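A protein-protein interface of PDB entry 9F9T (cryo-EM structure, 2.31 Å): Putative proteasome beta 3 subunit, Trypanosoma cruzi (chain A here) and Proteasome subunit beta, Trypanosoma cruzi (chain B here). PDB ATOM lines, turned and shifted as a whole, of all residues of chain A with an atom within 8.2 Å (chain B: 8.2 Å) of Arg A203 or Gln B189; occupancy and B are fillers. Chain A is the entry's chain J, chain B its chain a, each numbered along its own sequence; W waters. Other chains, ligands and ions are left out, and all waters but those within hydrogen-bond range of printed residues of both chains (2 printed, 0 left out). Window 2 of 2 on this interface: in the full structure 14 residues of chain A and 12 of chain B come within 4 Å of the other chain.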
ATOM      1  N   ASN A  26      -6.274 -33.702 -17.979  1.00  0.00           N
ATOM      2  CA  ASN A  26      -4.843 -34.034 -17.788  1.00  0.00           C
ATOM      3  C   ASN A  26      -4.562 -34.798 -16.495  1.00  0.00           C
ATOM      4  O   ASN A  26      -3.436 -35.081 -16.153  1.00  0.00           O
ATOM      5  CB  ASN A  26      -3.994 -32.795 -17.586  1.00  0.00           C
ATOM      6  CG  ASN A  26      -3.695 -32.040 -18.841  1.00  0.00           C
ATOM      7  OD1 ASN A  26      -3.194 -32.586 -19.821  1.00  0.00           O
ATOM      8  ND2 ASN A  26      -4.093 -30.791 -18.852  1.00  0.00           N
ATOM      9  N   MET A  37      -0.569 -34.328 -12.858  1.00  0.00           N
ATOM     10  CA  MET A  37      -1.489 -33.390 -13.470  1.00  0.00           C
ATOM     11  C   MET A  37      -1.123 -33.108 -14.919  1.00  0.00           C
ATOM     12  O   MET A  37      -1.516 -32.069 -15.402  1.00  0.00           O
ATOM     13  CB  MET A  37      -1.481 -32.062 -12.717  1.00  0.00           C
ATOM     14  CG  MET A  37      -2.021 -32.139 -11.320  1.00  0.00           C
ATOM     15  SD  MET A  37      -0.854 -32.799  -9.979  1.00  0.00           S
ATOM     16  CE  MET A  37      -1.854 -32.544  -8.498  1.00  0.00           C
ATOM     17  N   GLN A 169     -14.935 -24.961 -23.815  1.00  0.00           N
ATOM     18  CA  GLN A 169     -15.886 -24.612 -22.778  1.00  0.00           C
ATOM     19  C   GLN A 169     -16.571 -25.847 -22.260  1.00  0.00           C
ATOM     20  O   GLN A 169     -16.772 -25.938 -21.071  1.00  0.00           O
ATOM     21  CB  GLN A 169     -16.967 -23.652 -23.245  1.00  0.00           C
ATOM     22  CG  GLN A 169     -16.363 -22.315 -23.585  1.00  0.00           C
ATOM     23  CD  GLN A 169     -15.728 -21.688 -22.371  1.00  0.00           C
ATOM     24  OE1 GLN A 169     -16.308 -21.625 -21.279  1.00  0.00           O
ATOM     25  NE2 GLN A 169     -14.521 -21.179 -22.552  1.00  0.00           N
ATOM     26  N   LEU A 172     -14.057 -27.851 -19.937  1.00  0.00           N
ATOM     27  CA  LEU A 172     -13.850 -27.177 -18.649  1.00  0.00           C
ATOM     28  C   LEU A 172     -15.087 -27.177 -17.709  1.00  0.00           C
ATOM     29  O   LEU A 172     -15.025 -27.585 -16.555  1.00  0.00           O
ATOM     30  CB  LEU A 172     -13.349 -25.766 -18.889  1.00  0.00           C
ATOM     31  CG  LEU A 172     -12.024 -25.717 -19.626  1.00  0.00           C
ATOM     32  CD1 LEU A 172     -11.617 -24.297 -19.936  1.00  0.00           C
ATOM     33  CD2 LEU A 172     -10.935 -26.466 -18.869  1.00  0.00           C
ATOM     34  N   SER A 173     -16.208 -26.685 -18.156  1.00  0.00           N
ATOM     35  CA  SER A 173     -17.396 -26.686 -17.334  1.00  0.00           C
ATOM     36  C   SER A 173     -17.715 -28.111 -16.884  1.00  0.00           C
ATOM     37  O   SER A 173     -18.208 -28.305 -15.785  1.00  0.00           O
ATOM     38  CB  SER A 173     -18.564 -26.029 -18.070  1.00  0.00           C
ATOM     39  OG  SER A 173     -18.113 -24.950 -18.908  1.00  0.00           O
ATOM     40  N   CYS A 175     -15.490 -30.725 -16.452  1.00  0.00           N
ATOM     41  CA  CYS A 175     -14.526 -31.198 -15.495  1.00  0.00           C
ATOM     42  C   CYS A 175     -14.713 -30.514 -14.160  1.00  0.00           C
ATOM     43  O   CYS A 175     -14.403 -31.162 -13.175  1.00  0.00           O
ATOM     44  CB  CYS A 175     -13.108 -31.107 -16.023  1.00  0.00           C
ATOM     45  SG  CYS A 175     -12.879 -32.349 -17.336  1.00  0.00           S
ATOM     46  N   ASP A 176     -15.259 -29.297 -14.116  1.00  0.00           N
ATOM     47  CA  ASP A 176     -15.375 -28.570 -12.864  1.00  0.00           C
ATOM     48  C   ASP A 176     -16.466 -29.074 -11.942  1.00  0.00           C
ATOM     49  O   ASP A 176     -16.553 -28.611 -10.838  1.00  0.00           O
ATOM     50  CB  ASP A 176     -15.584 -27.085 -13.114  1.00  0.00           C
ATOM     51  CG  ASP A 176     -14.242 -26.425 -13.408  1.00  0.00           C
ATOM     52  OD1 ASP A 176     -13.183 -27.023 -13.026  1.00  0.00           O
ATOM     53  OD2 ASP A 176     -14.239 -25.345 -14.062  1.00  0.00           O
ATOM     54  N   ARG A 177     -17.363 -29.919 -12.413  1.00  0.00           N
ATOM     55  CA  ARG A 177     -18.311 -30.554 -11.532  1.00  0.00           C
ATOM     56  C   ARG A 177     -17.915 -32.010 -11.300  1.00  0.00           C
ATOM     57  O   ARG A 177     -18.644 -32.740 -10.651  1.00  0.00           O
ATOM     58  CB  ARG A 177     -19.663 -30.394 -12.192  1.00  0.00           C
ATOM     59  CG  ARG A 177     -20.167 -28.956 -12.166  1.00  0.00           C
ATOM     60  CD  ARG A 177     -20.915 -28.832 -10.882  1.00  0.00           C
ATOM     61  NE  ARG A 177     -21.404 -27.512 -10.734  1.00  0.00           N
ATOM     62  CZ  ARG A 177     -21.995 -27.031  -9.651  1.00  0.00           C
ATOM     63  NH1 ARG A 177     -22.180 -27.753  -8.566  1.00  0.00           N
ATOM     64  NH2 ARG A 177     -22.505 -25.828  -9.728  1.00  0.00           N
ATOM     65  N   SER A 181     -11.625 -35.587 -12.837  1.00  0.00           N
ATOM     66  CA  SER A 181     -11.089 -35.170 -14.124  1.00  0.00           C
ATOM     67  C   SER A 181     -10.853 -33.671 -14.033  1.00  0.00           C
ATOM     68  O   SER A 181     -11.529 -32.983 -13.266  1.00  0.00           O
ATOM     69  CB  SER A 181     -11.999 -35.520 -15.301  1.00  0.00           C
ATOM     70  OG  SER A 181     -12.103 -36.920 -15.549  1.00  0.00           O
ATOM     71  N   GLY A 182      -9.838 -33.183 -14.677  1.00  0.00           N
ATOM     72  CA  GLY A 182      -9.507 -31.808 -14.425  1.00  0.00           C
ATOM     73  C   GLY A 182      -8.071 -31.511 -14.712  1.00  0.00           C
ATOM     74  O   GLY A 182      -7.500 -32.280 -15.470  1.00  0.00           O
ATOM     75  N   TYR A 183      -7.565 -30.432 -14.120  1.00  0.00           N
ATOM     76  CA  TYR A 183      -6.231 -29.894 -14.339  1.00  0.00           C
ATOM     77  C   TYR A 183      -6.034 -29.462 -15.799  1.00  0.00           C
ATOM     78  O   TYR A 183      -4.997 -29.663 -16.414  1.00  0.00           O
ATOM     79  CB  TYR A 183      -5.149 -30.858 -13.786  1.00  0.00           C
ATOM     80  CG  TYR A 183      -5.285 -31.065 -12.285  1.00  0.00           C
ATOM     81  CD1 TYR A 183      -4.724 -30.169 -11.383  1.00  0.00           C
ATOM     82  CD2 TYR A 183      -6.157 -32.010 -11.757  1.00  0.00           C
ATOM     83  CE1 TYR A 183      -4.873 -30.331 -10.017  1.00  0.00           C
ATOM     84  CE2 TYR A 183      -6.417 -32.115 -10.383  1.00  0.00           C
ATOM     85  CZ  TYR A 183      -5.727 -31.292  -9.506  1.00  0.00           C
ATOM     86  OH  TYR A 183      -5.935 -31.364  -8.148  1.00  0.00           O
ATOM     87  N   GLY A 184      -7.079 -28.840 -16.349  1.00  0.00           N
ATOM     88  CA  GLY A 184      -7.007 -28.222 -17.663  1.00  0.00           C
ATOM     89  C   GLY A 184      -6.999 -29.271 -18.760  1.00  0.00           C
ATOM     90  O   GLY A 184      -7.375 -30.395 -18.471  1.00  0.00           O
ATOM     91  N   ALA A 185      -6.609 -28.934 -19.983  1.00  0.00           N
ATOM     92  CA  ALA A 185      -6.868 -29.854 -21.071  1.00  0.00           C
ATOM     93  C   ALA A 185      -5.939 -29.658 -22.227  1.00  0.00           C
ATOM     94  O   ALA A 185      -5.238 -28.674 -22.334  1.00  0.00           O
ATOM     95  CB  ALA A 185      -8.248 -29.649 -21.574  1.00  0.00           C
ATOM     96  N   ILE A 200      -4.998 -25.931 -22.758  1.00  0.00           N
ATOM     97  CA  ILE A 200      -5.974 -24.993 -22.225  1.00  0.00           C
ATOM     98  C   ILE A 200      -5.812 -24.874 -20.725  1.00  0.00           C
ATOM     99  O   ILE A 200      -5.713 -25.884 -20.067  1.00  0.00           O
ATOM    100  CB  ILE A 200      -7.361 -25.583 -22.506  1.00  0.00           C
ATOM    101  CG1 ILE A 200      -7.522 -25.885 -23.989  1.00  0.00           C
ATOM    102  CG2 ILE A 200      -8.489 -24.727 -21.946  1.00  0.00           C
ATOM    103  CD1 ILE A 200      -8.801 -26.666 -24.247  1.00  0.00           C
ATOM    104  N   ASN A 201      -5.878 -23.681 -20.171  1.00  0.00           N
ATOM    105  CA  ASN A 201      -5.790 -23.532 -18.722  1.00  0.00           C
ATOM    106  C   ASN A 201      -7.069 -24.017 -18.027  1.00  0.00           C
ATOM    107  O   ASN A 201      -8.149 -23.907 -18.580  1.00  0.00           O
ATOM    108  CB  ASN A 201      -5.547 -22.080 -18.328  1.00  0.00           C
ATOM    109  CG  ASN A 201      -4.779 -21.967 -17.033  1.00  0.00           C
ATOM    110  OD1 ASN A 201      -3.863 -22.750 -16.782  1.00  0.00           O
ATOM    111  ND2 ASN A 201      -5.136 -20.994 -16.209  1.00  0.00           N
ATOM    112  N   GLY A 202      -6.942 -24.588 -16.820  1.00  0.00           N
ATOM    113  CA  GLY A 202      -8.110 -24.802 -15.976  1.00  0.00           C
ATOM    114  C   GLY A 202      -7.835 -24.703 -14.481  1.00  0.00           C
ATOM    115  O   GLY A 202      -6.763 -24.319 -14.031  1.00  0.00           O
ATOM    116  N   ARG A 203      -8.804 -25.114 -13.713  1.00  0.00           N
ATOM    117  CA  ARG A 203      -8.692 -25.051 -12.278  1.00  0.00           C
ATOM    118  C   ARG A 203      -7.605 -26.013 -11.782  1.00  0.00           C
ATOM    119  O   ARG A 203      -7.264 -26.993 -12.451  1.00  0.00           O
ATOM    120  CB  ARG A 203     -10.095 -25.326 -11.704  1.00  0.00           C
ATOM    121  CG  ARG A 203     -11.080 -24.154 -11.740  1.00  0.00           C
ATOM    122  CD  ARG A 203     -12.300 -24.536 -10.900  1.00  0.00           C
ATOM    123  NE  ARG A 203     -12.031 -24.552  -9.465  1.00  0.00           N
ATOM    124  CZ  ARG A 203     -11.731 -23.454  -8.780  1.00  0.00           C
ATOM    125  NH1 ARG A 203     -11.888 -22.265  -9.329  1.00  0.00           N
ATOM    126  NH2 ARG A 203     -11.277 -23.543  -7.541  1.00  0.00           N
ATOM    127  N   LYS A 204      -7.084 -25.712 -10.593  1.00  0.00           N
ATOM    128  CA  LYS A 204      -5.979 -26.426  -9.960  1.00  0.00           C
ATOM    129  C   LYS A 204      -6.465 -27.270  -8.791  1.00  0.00           C
ATOM    130  O   LYS A 204      -5.747 -27.519  -7.841  1.00  0.00           O
ATOM    131  CB  LYS A 204      -4.937 -25.416  -9.503  1.00  0.00           C
ATOM    132  CG  LYS A 204      -3.913 -25.081 -10.574  1.00  0.00           C
ATOM    133  CD  LYS A 204      -4.470 -24.840 -11.914  1.00  0.00           C
ATOM    134  CE  LYS A 204      -3.533 -24.093 -12.834  1.00  0.00           C
ATOM    135  NZ  LYS A 204      -4.330 -23.157 -13.682  1.00  0.00           N
ATOM    136  N   ASP A 205      -7.718 -27.700  -8.898  1.00  0.00           N
ATOM    137  CA  ASP A 205      -8.346 -28.666  -8.012  1.00  0.00           C
ATOM    138  C   ASP A 205      -9.124 -29.638  -8.945  1.00  0.00           C
ATOM    139  O   ASP A 205      -8.993 -29.445 -10.235  1.00  0.00           O
ATOM    140  CB  ASP A 205      -9.131 -27.907  -6.912  1.00  0.00           C
ATOM    141  CG  ASP A 205     -10.290 -26.981  -7.329  1.00  0.00           C
ATOM    142  OD1 ASP A 205     -10.754 -27.037  -8.534  1.00  0.00           O
ATOM    143  OD2 ASP A 205     -10.756 -26.190  -6.442  1.00  0.00           O
ATOM    144  OXT ASP A 205      -9.857 -30.553  -8.408  1.00  0.00           O
ATOM    145  N   ASP B 183     -23.609 -23.140 -14.892  1.00  0.00           N
ATOM    146  CA  ASP B 183     -22.352 -22.658 -14.373  1.00  0.00           C
ATOM    147  C   ASP B 183     -21.689 -21.852 -15.484  1.00  0.00           C
ATOM    148  O   ASP B 183     -21.463 -20.667 -15.320  1.00  0.00           O
ATOM    149  CB  ASP B 183     -21.425 -23.764 -13.850  1.00  0.00           C
ATOM    150  CG  ASP B 183     -21.754 -24.529 -12.553  1.00  0.00           C
ATOM    151  OD1 ASP B 183     -22.297 -23.942 -11.600  1.00  0.00           O
ATOM    152  OD2 ASP B 183     -21.312 -25.726 -12.477  1.00  0.00           O
ATOM    153  N   CYS B 184     -21.471 -22.470 -16.636  1.00  0.00           N
ATOM    154  CA  CYS B 184     -20.929 -21.812 -17.825  1.00  0.00           C
ATOM    155  C   CYS B 184     -21.622 -20.475 -18.145  1.00  0.00           C
ATOM    156  O   CYS B 184     -20.954 -19.450 -18.238  1.00  0.00           O
ATOM    157  CB  CYS B 184     -20.940 -22.767 -19.032  1.00  0.00           C
ATOM    158  SG  CYS B 184     -20.012 -22.206 -20.497  1.00  0.00           S
ATOM    159  N   LEU B 185     -22.903 -20.440 -18.404  1.00  0.00           N
ATOM    160  CA  LEU B 185     -23.478 -19.244 -19.039  1.00  0.00           C
ATOM    161  C   LEU B 185     -23.626 -18.098 -18.033  1.00  0.00           C
ATOM    162  O   LEU B 185     -23.508 -16.948 -18.421  1.00  0.00           O
ATOM    163  CB  LEU B 185     -24.844 -19.577 -19.659  1.00  0.00           C
ATOM    164  CG  LEU B 185     -24.845 -20.737 -20.668  1.00  0.00           C
ATOM    165  CD1 LEU B 185     -26.257 -21.042 -21.200  1.00  0.00           C
ATOM    166  CD2 LEU B 185     -23.874 -20.454 -21.829  1.00  0.00           C
ATOM    167  N   LEU B 186     -23.868 -18.401 -16.744  1.00  0.00           N
ATOM    168  CA  LEU B 186     -24.065 -17.380 -15.713  1.00  0.00           C
ATOM    169  C   LEU B 186     -22.770 -16.961 -15.035  1.00  0.00           C
ATOM    170  O   LEU B 186     -22.644 -15.787 -14.727  1.00  0.00           O
ATOM    171  CB  LEU B 186     -25.009 -17.899 -14.646  1.00  0.00           C
ATOM    172  CG  LEU B 186     -26.366 -18.287 -15.187  1.00  0.00           C
ATOM    173  CD1 LEU B 186     -27.115 -19.122 -14.167  1.00  0.00           C
ATOM    174  CD2 LEU B 186     -27.127 -17.024 -15.610  1.00  0.00           C
ATOM    175  N   THR B 187     -21.794 -17.836 -14.811  1.00  0.00           N
ATOM    176  CA  THR B 187     -20.623 -17.355 -14.074  1.00  0.00           C
ATOM    177  C   THR B 187     -19.445 -17.025 -14.991  1.00  0.00           C
ATOM    178  O   THR B 187     -18.618 -16.209 -14.588  1.00  0.00           O
ATOM    179  CB  THR B 187     -20.275 -18.262 -12.870  1.00  0.00           C
ATOM    180  OG1 THR B 187     -19.905 -19.589 -13.237  1.00  0.00           O
ATOM    181  CG2 THR B 187     -21.449 -18.392 -11.919  1.00  0.00           C
ATOM    182  N   ARG B 188     -19.314 -17.747 -16.121  1.00  0.00           N
ATOM    183  CA  ARG B 188     -18.321 -17.524 -17.183  1.00  0.00           C
ATOM    184  C   ARG B 188     -16.877 -17.532 -16.656  1.00  0.00           C
ATOM    185  O   ARG B 188     -16.136 -16.576 -16.844  1.00  0.00           O
ATOM    186  CB  ARG B 188     -18.628 -16.195 -17.888  1.00  0.00           C
ATOM    187  CG  ARG B 188     -20.114 -15.919 -18.111  1.00  0.00           C
ATOM    188  CD  ARG B 188     -20.408 -14.614 -18.813  1.00  0.00           C
ATOM    189  NE  ARG B 188     -20.135 -14.686 -20.234  1.00  0.00           N
ATOM    190  CZ  ARG B 188     -20.329 -13.683 -21.081  1.00  0.00           C
ATOM    191  NH1 ARG B 188     -20.132 -13.866 -22.374  1.00  0.00           N
ATOM    192  NH2 ARG B 188     -20.734 -12.504 -20.633  1.00  0.00           N
ATOM    193  N   GLN B 189     -16.484 -18.597 -15.950  1.00  0.00           N
ATOM    194  CA  GLN B 189     -15.241 -18.572 -15.206  1.00  0.00           C
ATOM    195  C   GLN B 189     -14.080 -18.854 -16.165  1.00  0.00           C
ATOM    196  O   GLN B 189     -12.985 -18.356 -15.946  1.00  0.00           O
ATOM    197  CB  GLN B 189     -15.301 -19.485 -13.970  1.00  0.00           C
ATOM    198  CG  GLN B 189     -14.378 -20.704 -14.024  1.00  0.00           C
ATOM    199  CD  GLN B 189     -13.991 -21.296 -12.679  1.00  0.00           C
ATOM    200  OE1 GLN B 189     -12.825 -21.254 -12.268  1.00  0.00           O
ATOM    201  NE2 GLN B 189     -14.964 -21.907 -12.013  1.00  0.00           N
ATOM    202  N   HIS B 190     -14.337 -19.562 -17.274  1.00  0.00           N
ATOM    203  CA  HIS B 190     -13.288 -19.901 -18.233  1.00  0.00           C
ATOM    204  C   HIS B 190     -13.397 -19.052 -19.501  1.00  0.00           C
ATOM    205  O   HIS B 190     -13.107 -19.567 -20.589  1.00  0.00           O
ATOM    206  CB  HIS B 190     -13.280 -21.406 -18.571  1.00  0.00           C
ATOM    207  CG  HIS B 190     -13.187 -22.281 -17.366  1.00  0.00           C
ATOM    208  ND1 HIS B 190     -12.123 -22.230 -16.484  1.00  0.00           N
ATOM    209  CD2 HIS B 190     -14.043 -23.179 -16.866  1.00  0.00           C
ATOM    210  CE1 HIS B 190     -12.330 -23.088 -15.496  1.00  0.00           C
ATOM    211  NE2 HIS B 190     -13.483 -23.671 -15.702  1.00  0.00           N
ATOM    212  N   MET B 191     -13.758 -17.757 -19.331  1.00  0.00           N
ATOM    213  CA  MET B 191     -13.860 -16.793 -20.429  1.00  0.00           C
ATOM    214  C   MET B 191     -13.083 -15.529 -20.090  1.00  0.00           C
ATOM    215  O   MET B 191     -12.571 -15.414 -18.976  1.00  0.00           O
ATOM    216  CB  MET B 191     -15.318 -16.450 -20.714  1.00  0.00           C
ATOM    217  CG  MET B 191     -16.072 -17.678 -21.176  1.00  0.00           C
ATOM    218  SD  MET B 191     -17.778 -17.377 -21.630  1.00  0.00           S
ATOM    219  CE  MET B 191     -18.516 -18.974 -21.270  1.00  0.00           C
ATOM    220  N   VAL B 192     -12.996 -14.601 -21.062  1.00  0.00           N
ATOM    221  CA  VAL B 192     -12.224 -13.368 -20.926  1.00  0.00           C
ATOM    222  C   VAL B 192     -13.166 -12.151 -20.747  1.00  0.00           C
ATOM    223  O   VAL B 192     -14.373 -12.214 -21.146  1.00  0.00           O
ATOM    224  CB  VAL B 192     -11.253 -13.218 -22.124  1.00  0.00           C
ATOM    225  CG1 VAL B 192     -10.156 -12.205 -21.844  1.00  0.00           C
ATOM    226  CG2 VAL B 192     -10.619 -14.543 -22.544  1.00  0.00           C
HETATM  227  O   HOH W   1     -16.728 -20.848 -18.473  1.00  0.00           O
HETATM  228  O   HOH W   2     -11.569 -26.027 -14.919  1.00  0.00           O
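Water W2 lies within hydrogen-bond range of OD1 of Asp A176 (2.7 Å), NE2 of His B190 (3.1 Å) and N of Arg A203 (3.2 Å). Water W1 lies within hydrogen-bond range of the side-chain amide oxygen of Gln A169, the backbone NH of His B190 and the backbone NH of Gln B189.
Of chain B, only Gln B189 (3.2 Å) comes within 4 Å of Arg A203. Of chain A, only Arg A203 (3.2 Å) comes within 4 Å of Gln B189. No residue of chain B comes within 4 Å of Gly A202. Of the printed residues of chain A, His B190 touches Gln A169, Leu A172 and Asp A176. Of the printed residues of chain A, Asp B183 touches Arg A177. Of the printed residues of chain B, Gln A169 touches Cys B184, His B190 and Met B191. Printed residues of chain B within 4 Å of Arg A177: Asp B183. Of the printed residues of chain B, Ser A173 touches Cys B184 (3.6 Å). Leu B186 touches none of the printed residues of chain A. The nearest residue of chain A that does not touch Gln B189 is Asp A176 (4.1 Å). The nearest printed residue of chain A that does not touch Cys B184 is Leu A172 (7.4 Å).
Cys B184 touches Gln A169. Met B191 touches Gln A169. Leu A172 touches His B190 (CB to CD2, 3.4 Å).
OG of Ser A173 sits at hydrogen-bond distance from O of Gln A169 (2.7 Å). The backbone carbonyl oxygen (O) of Asp B183 lies within hydrogen-bond range of the side-chain hydroxyl (OG1) of Thr B187 (2.8 Å). NH2 of Arg A203 is in salt-bridge range of OD2 of Asp A205, at 2.9 Å.
Of the 10 printed residues of chain B, 5 touch a printed residue of chain A. Hydrophobic or aromatic side chains of chain B that line the printed part of chain A: His B190 and Met B191. Of the 19 printed residues of chain A, 6 touch a printed residue of chain B. Hydrophobic or aromatic side chains of chain A that line the printed part of chain B: Leu A172. Among the printed residues, 8 pairs touch across the chains. Among the printed residues, Asp or Glu carboxylates within 4 Å of a Lys or Arg side-chain nitrogen of the other chain: Arg A177 with Asp B183 (2.5 Å).
The side-chain amide nitrogen (NE2) of Gln A169 is in hydrogen-bond range of the backbone carbonyl oxygen (O) of His B190, at 2.9 Å. The side-chain carboxylate (OD2) of Asp A176 sits at hydrogen-bond distance from a ring nitrogen (NE2) of His B190 (2.5 Å). The side-chain sulfur (SG) of Cys B184 lies close to the side-chain hydroxyl (OG) of Ser A173, 3.7 Å away. NH1 of Arg A203 lies within hydrogen-bond range of OE1 of Gln B189 (3.2 Å). The side-chain carboxylate (OD2) of Asp B183 lies within salt-bridge range of the guanidinium group (NE) of Arg A177, at 2.5 Å.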
